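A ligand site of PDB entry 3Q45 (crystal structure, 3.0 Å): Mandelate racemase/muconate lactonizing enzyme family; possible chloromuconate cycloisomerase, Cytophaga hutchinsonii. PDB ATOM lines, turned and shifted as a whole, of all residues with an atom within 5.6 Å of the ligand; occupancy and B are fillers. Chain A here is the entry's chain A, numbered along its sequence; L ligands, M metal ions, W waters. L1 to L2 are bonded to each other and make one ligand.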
ATOM      1  N   PHE A  19      23.066 -16.087  -9.650  1.00  0.00           N
ATOM      2  CA  PHE A  19      23.855 -17.208  -9.170  1.00  0.00           C
ATOM      3  C   PHE A  19      22.989 -18.457  -9.239  1.00  0.00           C
ATOM      4  O   PHE A  19      21.901 -18.490  -8.694  1.00  0.00           O
ATOM      5  CB  PHE A  19      24.324 -16.918  -7.737  1.00  0.00           C
ATOM      6  CG  PHE A  19      25.179 -17.986  -7.140  1.00  0.00           C
ATOM      7  CD1 PHE A  19      26.457 -18.203  -7.596  1.00  0.00           C
ATOM      8  CD2 PHE A  19      24.714 -18.746  -6.072  1.00  0.00           C
ATOM      9  CE1 PHE A  19      27.250 -19.180  -7.026  1.00  0.00           C
ATOM     10  CE2 PHE A  19      25.506 -19.735  -5.508  1.00  0.00           C
ATOM     11  CZ  PHE A  19      26.764 -19.955  -5.983  1.00  0.00           C
ATOM     12  N   ILE A  21      22.511 -22.709  -9.066  1.00  0.00           N
ATOM     13  CA  ILE A  21      22.913 -24.057  -8.687  1.00  0.00           C
ATOM     14  C   ILE A  21      21.785 -25.024  -8.972  1.00  0.00           C
ATOM     15  O   ILE A  21      20.692 -24.601  -9.354  1.00  0.00           O
ATOM     16  CB  ILE A  21      23.307 -24.152  -7.207  1.00  0.00           C
ATOM     17  CG1 ILE A  21      22.127 -23.829  -6.309  1.00  0.00           C
ATOM     18  CG2 ILE A  21      24.484 -23.227  -6.912  1.00  0.00           C
ATOM     19  CD1 ILE A  21      22.391 -24.092  -4.847  1.00  0.00           C
ATOM     20  N   PHE A  51      20.007 -19.530   3.464  1.00  0.00           N
ATOM     21  CA  PHE A  51      19.776 -20.182   2.174  1.00  0.00           C
ATOM     22  C   PHE A  51      18.636 -21.166   2.343  1.00  0.00           C
ATOM     23  O   PHE A  51      18.826 -22.247   2.897  1.00  0.00           O
ATOM     24  CB  PHE A  51      21.061 -20.899   1.725  1.00  0.00           C
ATOM     25  CG  PHE A  51      21.121 -21.156   0.245  1.00  0.00           C
ATOM     26  CD1 PHE A  51      20.596 -22.317  -0.280  1.00  0.00           C
ATOM     27  CD2 PHE A  51      21.700 -20.234  -0.603  1.00  0.00           C
ATOM     28  CE1 PHE A  51      20.639 -22.549  -1.634  1.00  0.00           C
ATOM     29  CE2 PHE A  51      21.734 -20.455  -1.961  1.00  0.00           C
ATOM     30  CZ  PHE A  51      21.210 -21.604  -2.480  1.00  0.00           C
ATOM     31  N   ILE A  54      18.610 -25.078   2.000  1.00  0.00           N
ATOM     32  CA  ILE A  54      19.665 -25.799   2.703  1.00  0.00           C
ATOM     33  C   ILE A  54      19.628 -25.569   4.185  1.00  0.00           C
ATOM     34  O   ILE A  54      19.718 -26.494   4.983  1.00  0.00           O
ATOM     35  CB  ILE A  54      21.078 -25.463   2.156  1.00  0.00           C
ATOM     36  CG1 ILE A  54      21.128 -25.672   0.647  1.00  0.00           C
ATOM     37  CG2 ILE A  54      22.134 -26.319   2.843  1.00  0.00           C
ATOM     38  CD1 ILE A  54      22.452 -25.722   0.091  1.00  0.00           C
ATOM     39  N   ASP A 133      38.738 -20.418  -5.051  1.00  0.00           N
ATOM     40  CA  ASP A 133      38.287 -20.781  -6.376  1.00  0.00           C
ATOM     41  C   ASP A 133      37.304 -19.705  -6.823  1.00  0.00           C
ATOM     42  O   ASP A 133      37.116 -18.712  -6.140  1.00  0.00           O
ATOM     43  CB  ASP A 133      37.597 -22.141  -6.359  1.00  0.00           C
ATOM     44  CG  ASP A 133      36.468 -22.205  -5.359  1.00  0.00           C
ATOM     45  OD1 ASP A 133      36.323 -23.249  -4.685  1.00  0.00           O
ATOM     46  OD2 ASP A 133      35.723 -21.212  -5.228  1.00  0.00           O
ATOM     47  N   THR A 135      33.306 -19.561  -9.021  1.00  0.00           N
ATOM     48  CA  THR A 135      32.221 -20.505  -9.282  1.00  0.00           C
ATOM     49  C   THR A 135      31.512 -20.239 -10.598  1.00  0.00           C
ATOM     50  O   THR A 135      31.032 -19.120 -10.842  1.00  0.00           O
ATOM     51  CB  THR A 135      31.182 -20.524  -8.107  1.00  0.00           C
ATOM     52  OG1 THR A 135      31.760 -21.102  -6.935  1.00  0.00           O
ATOM     53  CG2 THR A 135      29.945 -21.304  -8.469  1.00  0.00           C
ATOM     54  N   LYS A 160      35.339 -23.740  -9.681  1.00  0.00           N
ATOM     55  CA  LYS A 160      34.331 -24.620  -9.105  1.00  0.00           C
ATOM     56  C   LYS A 160      33.101 -24.615  -9.982  1.00  0.00           C
ATOM     57  O   LYS A 160      32.471 -23.561 -10.194  1.00  0.00           O
ATOM     58  CB  LYS A 160      33.988 -24.181  -7.688  1.00  0.00           C
ATOM     59  CG  LYS A 160      32.831 -24.915  -7.070  1.00  0.00           C
ATOM     60  CD  LYS A 160      32.784 -24.678  -5.570  1.00  0.00           C
ATOM     61  CE  LYS A 160      31.426 -25.023  -4.985  1.00  0.00           C
ATOM     62  NZ  LYS A 160      31.396 -24.876  -3.516  1.00  0.00           N
ATOM     63  N   LYS A 162      29.273 -25.854 -11.007  1.00  0.00           N
ATOM     64  CA  LYS A 162      27.996 -26.323 -10.490  1.00  0.00           C
ATOM     65  C   LYS A 162      27.361 -27.300 -11.459  1.00  0.00           C
ATOM     66  O   LYS A 162      26.854 -26.918 -12.513  1.00  0.00           O
ATOM     67  CB  LYS A 162      27.039 -25.161 -10.226  1.00  0.00           C
ATOM     68  CG  LYS A 162      27.437 -24.261  -9.063  1.00  0.00           C
ATOM     69  CD  LYS A 162      27.454 -25.035  -7.770  1.00  0.00           C
ATOM     70  CE  LYS A 162      27.850 -24.150  -6.591  1.00  0.00           C
ATOM     71  NZ  LYS A 162      27.672 -24.809  -5.295  1.00  0.00           N
ATOM     72  N   ASP A 190      30.419 -29.431  -7.993  1.00  0.00           N
ATOM     73  CA  ASP A 190      29.451 -29.421  -6.906  1.00  0.00           C
ATOM     74  C   ASP A 190      28.037 -29.670  -7.454  1.00  0.00           C
ATOM     75  O   ASP A 190      27.548 -28.908  -8.305  1.00  0.00           O
ATOM     76  CB  ASP A 190      29.504 -28.064  -6.202  1.00  0.00           C
ATOM     77  CG  ASP A 190      28.720 -28.011  -4.923  1.00  0.00           C
ATOM     78  OD1 ASP A 190      27.917 -28.928  -4.642  1.00  0.00           O
ATOM     79  OD2 ASP A 190      28.900 -27.020  -4.187  1.00  0.00           O
ATOM     80  N   ASN A 192      25.216 -30.238  -5.478  1.00  0.00           N
ATOM     81  CA  ASN A 192      24.175 -29.766  -4.588  1.00  0.00           C
ATOM     82  C   ASN A 192      23.015 -30.728  -4.566  1.00  0.00           C
ATOM     83  O   ASN A 192      21.866 -30.346  -4.812  1.00  0.00           O
ATOM     84  CB  ASN A 192      23.684 -28.374  -4.987  1.00  0.00           C
ATOM     85  CG  ASN A 192      24.710 -27.305  -4.710  1.00  0.00           C
ATOM     86  OD1 ASN A 192      25.162 -27.150  -3.570  1.00  0.00           O
ATOM     87  ND2 ASN A 192      25.088 -26.573  -5.755  1.00  0.00           N
ATOM     88  N   GLU A 216      31.452 -32.142  -4.624  1.00  0.00           N
ATOM     89  CA  GLU A 216      30.693 -31.841  -3.429  1.00  0.00           C
ATOM     90  C   GLU A 216      29.289 -32.406  -3.539  1.00  0.00           C
ATOM     91  O   GLU A 216      28.637 -32.277  -4.570  1.00  0.00           O
ATOM     92  CB  GLU A 216      30.629 -30.328  -3.205  1.00  0.00           C
ATOM     93  CG  GLU A 216      31.874 -29.708  -2.627  1.00  0.00           C
ATOM     94  CD  GLU A 216      31.787 -28.198  -2.564  1.00  0.00           C
ATOM     95  OE1 GLU A 216      30.806 -27.697  -2.006  1.00  0.00           O
ATOM     96  OE2 GLU A 216      32.704 -27.515  -3.079  1.00  0.00           O
ATOM     97  N   ASP A 241      28.940 -31.806   1.776  1.00  0.00           N
ATOM     98  CA  ASP A 241      28.603 -30.436   2.132  1.00  0.00           C
ATOM     99  C   ASP A 241      27.326 -30.403   2.959  1.00  0.00           C
ATOM    100  O   ASP A 241      27.378 -30.360   4.181  1.00  0.00           O
ATOM    101  CB  ASP A 241      28.468 -29.568   0.880  1.00  0.00           C
ATOM    102  CG  ASP A 241      28.329 -28.086   1.226  1.00  0.00           C
ATOM    103  OD1 ASP A 241      27.844 -27.741   2.328  1.00  0.00           O
ATOM    104  OD2 ASP A 241      28.718 -27.267   0.367  1.00  0.00           O
ATOM    105  N   GLU A 242      26.173 -30.407   2.302  1.00  0.00           N
ATOM    106  CA  GLU A 242      24.909 -30.410   3.010  1.00  0.00           C
ATOM    107  C   GLU A 242      24.817 -31.587   3.961  1.00  0.00           C
ATOM    108  O   GLU A 242      24.137 -31.520   4.958  1.00  0.00           O
ATOM    109  CB  GLU A 242      23.728 -30.442   2.039  1.00  0.00           C
ATOM    110  CG  GLU A 242      23.513 -29.185   1.212  1.00  0.00           C
ATOM    111  CD  GLU A 242      24.330 -29.166  -0.072  1.00  0.00           C
ATOM    112  OE1 GLU A 242      25.561 -29.241   0.011  1.00  0.00           O
ATOM    113  OE2 GLU A 242      23.728 -29.052  -1.161  1.00  0.00           O
ATOM    114  N   ASN A 263      33.177 -30.145   3.404  1.00  0.00           N
ATOM    115  CA  ASN A 263      33.070 -28.706   3.175  1.00  0.00           C
ATOM    116  C   ASN A 263      32.500 -28.018   4.419  1.00  0.00           C
ATOM    117  O   ASN A 263      31.322 -28.110   4.711  1.00  0.00           O
ATOM    118  CB  ASN A 263      32.190 -28.417   1.959  1.00  0.00           C
ATOM    119  CG  ASN A 263      32.154 -26.944   1.621  1.00  0.00           C
ATOM    120  OD1 ASN A 263      32.508 -26.119   2.427  1.00  0.00           O
ATOM    121  ND2 ASN A 263      31.736 -26.617   0.405  1.00  0.00           N
ATOM    122  N   LYS A 265      31.323 -25.045   6.791  1.00  0.00           N
ATOM    123  CA  LYS A 265      30.703 -23.736   6.704  1.00  0.00           C
ATOM    124  C   LYS A 265      30.186 -23.324   8.099  1.00  0.00           C
ATOM    125  O   LYS A 265      29.501 -24.088   8.771  1.00  0.00           O
ATOM    126  CB  LYS A 265      29.547 -23.741   5.692  1.00  0.00           C
ATOM    127  CG  LYS A 265      29.910 -24.143   4.278  1.00  0.00           C
ATOM    128  CD  LYS A 265      28.780 -23.837   3.324  1.00  0.00           C
ATOM    129  CE  LYS A 265      28.776 -24.766   2.121  1.00  0.00           C
ATOM    130  NZ  LYS A 265      28.772 -24.021   0.819  1.00  0.00           N
ATOM    131  N   GLN A 290      37.660 -28.331   3.120  1.00  0.00           N
ATOM    132  CA  GLN A 290      37.503 -27.108   2.363  1.00  0.00           C
ATOM    133  C   GLN A 290      36.631 -26.209   3.212  1.00  0.00           C
ATOM    134  O   GLN A 290      35.613 -26.659   3.685  1.00  0.00           O
ATOM    135  CB  GLN A 290      36.824 -27.391   1.021  1.00  0.00           C
ATOM    136  CG  GLN A 290      36.401 -26.180   0.231  1.00  0.00           C
ATOM    137  CD  GLN A 290      35.724 -26.560  -1.094  1.00  0.00           C
ATOM    138  OE1 GLN A 290      34.526 -26.316  -1.296  1.00  0.00           O
ATOM    139  NE2 GLN A 290      36.481 -27.165  -1.995  1.00  0.00           N
ATOM    140  N   GLY A 293      31.117 -21.243   2.226  1.00  0.00           N
ATOM    141  CA  GLY A 293      30.055 -20.413   2.752  1.00  0.00           C
ATOM    142  C   GLY A 293      28.868 -20.353   1.821  1.00  0.00           C
ATOM    143  O   GLY A 293      28.701 -21.199   0.972  1.00  0.00           O
ATOM    144  N   PHE A 294      28.022 -19.345   1.991  1.00  0.00           N
ATOM    145  CA  PHE A 294      26.858 -19.158   1.135  1.00  0.00           C
ATOM    146  C   PHE A 294      26.965 -17.818   0.422  1.00  0.00           C
ATOM    147  O   PHE A 294      27.801 -17.674  -0.459  1.00  0.00           O
ATOM    148  CB  PHE A 294      25.552 -19.316   1.936  1.00  0.00           C
ATOM    149  CG  PHE A 294      25.334 -20.714   2.427  1.00  0.00           C
ATOM    150  CD1 PHE A 294      24.597 -21.619   1.681  1.00  0.00           C
ATOM    151  CD2 PHE A 294      25.906 -21.147   3.598  1.00  0.00           C
ATOM    152  CE1 PHE A 294      24.421 -22.920   2.130  1.00  0.00           C
ATOM    153  CE2 PHE A 294      25.730 -22.477   4.043  1.00  0.00           C
ATOM    154  CZ  PHE A 294      24.987 -23.346   3.307  1.00  0.00           C
ATOM    155  N   LEU A 295      26.131 -16.842   0.759  1.00  0.00           N
ATOM    156  CA  LEU A 295      26.271 -15.551   0.103  1.00  0.00           C
ATOM    157  C   LEU A 295      26.611 -14.455   1.085  1.00  0.00           C
ATOM    158  O   LEU A 295      26.183 -13.322   0.926  1.00  0.00           O
ATOM    159  CB  LEU A 295      25.040 -15.185  -0.729  1.00  0.00           C
ATOM    160  CG  LEU A 295      25.012 -15.851  -2.111  1.00  0.00           C
ATOM    161  CD1 LEU A 295      24.803 -17.342  -1.969  1.00  0.00           C
ATOM    162  CD2 LEU A 295      23.931 -15.271  -2.955  1.00  0.00           C
ATOM    163  N   PHE A 301      32.866 -14.034   5.294  1.00  0.00           N
ATOM    164  CA  PHE A 301      33.995 -14.795   4.809  1.00  0.00           C
ATOM    165  C   PHE A 301      35.290 -14.460   5.523  1.00  0.00           C
ATOM    166  O   PHE A 301      36.229 -15.247   5.481  1.00  0.00           O
ATOM    167  CB  PHE A 301      34.135 -14.677   3.298  1.00  0.00           C
ATOM    168  CG  PHE A 301      33.149 -15.509   2.538  1.00  0.00           C
ATOM    169  CD1 PHE A 301      33.339 -16.856   2.368  1.00  0.00           C
ATOM    170  CD2 PHE A 301      32.029 -14.948   2.003  1.00  0.00           C
ATOM    171  CE1 PHE A 301      32.440 -17.606   1.697  1.00  0.00           C
ATOM    172  CE2 PHE A 301      31.136 -15.705   1.326  1.00  0.00           C
ATOM    173  CZ  PHE A 301      31.352 -17.037   1.169  1.00  0.00           C
ATOM    174  N   ASP A 318      36.721 -21.811  -0.679  1.00  0.00           N
ATOM    175  CA  ASP A 318      35.658 -21.347  -1.580  1.00  0.00           C
ATOM    176  C   ASP A 318      35.051 -20.049  -1.016  1.00  0.00           C
ATOM    177  O   ASP A 318      34.115 -20.073  -0.240  1.00  0.00           O
ATOM    178  CB  ASP A 318      34.596 -22.442  -1.754  1.00  0.00           C
ATOM    179  CG  ASP A 318      33.465 -22.046  -2.694  1.00  0.00           C
ATOM    180  OD1 ASP A 318      32.349 -22.542  -2.501  1.00  0.00           O
ATOM    181  OD2 ASP A 318      33.674 -21.237  -3.623  1.00  0.00           O
ATOM    182  N   PHE A 319      35.621 -18.909  -1.388  1.00  0.00           N
ATOM    183  CA  PHE A 319      35.261 -17.631  -0.757  1.00  0.00           C
ATOM    184  C   PHE A 319      34.855 -16.618  -1.802  1.00  0.00           C
ATOM    185  O   PHE A 319      35.135 -15.450  -1.659  1.00  0.00           O
ATOM    186  CB  PHE A 319      36.445 -17.028   0.019  1.00  0.00           C
ATOM    187  CG  PHE A 319      36.869 -17.847   1.211  1.00  0.00           C
ATOM    188  CD1 PHE A 319      36.038 -18.788   1.760  1.00  0.00           C
ATOM    189  CD2 PHE A 319      38.102 -17.643   1.790  1.00  0.00           C
ATOM    190  CE1 PHE A 319      36.439 -19.516   2.856  1.00  0.00           C
ATOM    191  CE2 PHE A 319      38.498 -18.352   2.898  1.00  0.00           C
ATOM    192  CZ  PHE A 319      37.679 -19.287   3.434  1.00  0.00           C
ATOM    193  N   ASP A 320      34.189 -17.065  -2.860  1.00  0.00           N
ATOM    194  CA  ASP A 320      34.072 -16.229  -4.053  1.00  0.00           C
ATOM    195  C   ASP A 320      32.884 -15.277  -4.094  1.00  0.00           C
ATOM    196  O   ASP A 320      32.993 -14.189  -4.628  1.00  0.00           O
ATOM    197  CB  ASP A 320      34.084 -17.070  -5.320  1.00  0.00           C
ATOM    198  CG  ASP A 320      32.925 -18.044  -5.399  1.00  0.00           C
ATOM    199  OD1 ASP A 320      32.393 -18.465  -4.337  1.00  0.00           O
ATOM    200  OD2 ASP A 320      32.539 -18.414  -6.523  1.00  0.00           O
ATOM    201  N   THR A 321      31.769 -15.669  -3.514  1.00  0.00           N
ATOM    202  CA  THR A 321      30.521 -14.942  -3.695  1.00  0.00           C
ATOM    203  C   THR A 321      30.589 -13.453  -3.419  1.00  0.00           C
ATOM    204  O   THR A 321      29.895 -12.682  -4.061  1.00  0.00           O
ATOM    205  CB  THR A 321      29.384 -15.541  -2.879  1.00  0.00           C
ATOM    206  OG1 THR A 321      29.895 -16.010  -1.640  1.00  0.00           O
ATOM    207  CG2 THR A 321      28.755 -16.693  -3.616  1.00  0.00           C
HETATM  208  N1  LIG L   1      31.096 -20.905  -4.257  1.00  0.00           N
HETATM  209  C1  LIG L   1      29.907 -20.407  -3.497  1.00  0.00           C
HETATM  210  C2  LIG L   1      30.341 -19.761  -2.189  1.00  0.00           C
HETATM  211  C3  LIG L   1      28.902 -21.560  -3.260  1.00  0.00           C
HETATM  212  O1  LIG L   1      28.475 -22.206  -4.229  1.00  0.00           O
HETATM  213  N1  LG2 L   2      28.530 -21.806  -1.998  1.00  0.00           N
HETATM  214  C1  LG2 L   2      27.602 -22.874  -1.631  1.00  0.00           C
HETATM  215  C2  LG2 L   2      28.199 -24.285  -1.959  1.00  0.00           C
HETATM  216  O1  LG2 L   2      29.288 -24.692  -1.484  1.00  0.00           O
HETATM  217  C3  LG2 L   2      26.193 -22.663  -2.283  1.00  0.00           C
HETATM  218  C4  LG2 L   2      25.125 -23.469  -1.590  1.00  0.00           C
HETATM  219  C5  LG2 L   2      25.777 -21.235  -2.225  1.00  0.00           C
HETATM  220  O2  LG2 L   2      27.643 -25.086  -2.726  1.00  0.00           O
HETATM  221 MG    MG M   1      28.266 -27.580  -1.720  1.00  0.00          MG
HETATM  222  O   HOH W   1      31.240 -23.215  -0.201  1.00  0.00           O
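The backbone carbonyl oxygen of Phe 294 sits at hydrogen-bond distance from the side-chain hydroxyl of Thr 321. The side-chain amino group (NZ) of Lys 265 lies close to the side-chain carboxylate (OD2) of Asp 241. The side-chain amide oxygen (OD1) of Asn 192 sits close to the side-chain carboxylate (OE2) of Glu 242 (3.4 Å). OD2 of Asp 241 sits close to ND2 of Asn 263, 3.1 Å away. The side-chain carboxylate (OE2) of Glu 216 sits close to the side-chain amide oxygen (OE1) of Gln 290 (2.8 Å). OD1 of Asp 318 lies within salt-bridge range of NZ of Lys 160 (2.7 Å). The side-chain amino group of Lys 160 is in salt-bridge range of the side-chain carboxylate of Glu 216. The backbone NH (N) of Asn 192 sits at hydrogen-bond distance from the side-chain carboxylate (OD1) of Asp 190 (3.1 Å).
O1 of LG2 L2 lies close to OE1 of Glu 216. OD2 of Asp 241 sits close to O1 of LG2 L2, 3.2 Å away. Merely in contact with the ligand: Phe 19 (3.3 Å), Asn 263 (3.6 Å), Phe 294 (3.7 Å), Thr 321 (3.7 Å) and Ile 54 (3.9 Å). 16 residues have an atom within 4 Å of the ligand: Phe 19, Ile 54, Thr 135, Lys 160, Lys 162, Asp 190, Asn 192, Glu 216, Asp 241, Asn 263, Lys 265, Gly 293, Phe 294, Asp 318, Asp 320 and Thr 321. The nearest printed residue that does not touch the ligand is Leu 295 (4.02 Å).
OG1 of Thr 135 lies within hydrogen-bond range of N1 of LIG L1 (2.8 Å). N1 of LIG L1 is in salt-bridge range of OD1 of Asp 320, 2.8 Å away. The backbone carbonyl oxygen (O) of Gly 293 lies within hydrogen-bond range of a nitrogen (N1) of LG2 L2 (3.0 Å). The side-chain amino group (NZ) of Lys 162 is in salt-bridge range of an oxygen (O2) of LG2 L2 (2.6 Å). The side-chain carboxylate (OD2) of Asp 190 lies close to an oxygen (O2) of LG2 L2 (2.7 Å). The side-chain amino group (NZ) of Lys 160 lies within salt-bridge range of an oxygen (O1) of LG2 L2 (2.9 Å). An oxygen (O1) of LG2 L2 lies within salt-bridge range of the side-chain amino group (NZ) of Lys 265. An oxygen (O2) of LG2 L2 lies close to the side-chain amide oxygen (OD1) of Asn 192 (3.3 Å). A nitrogen (N1) of LIG L1 is in salt-bridge range of the side-chain carboxylate of Asp 318, at 2.7 Å.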
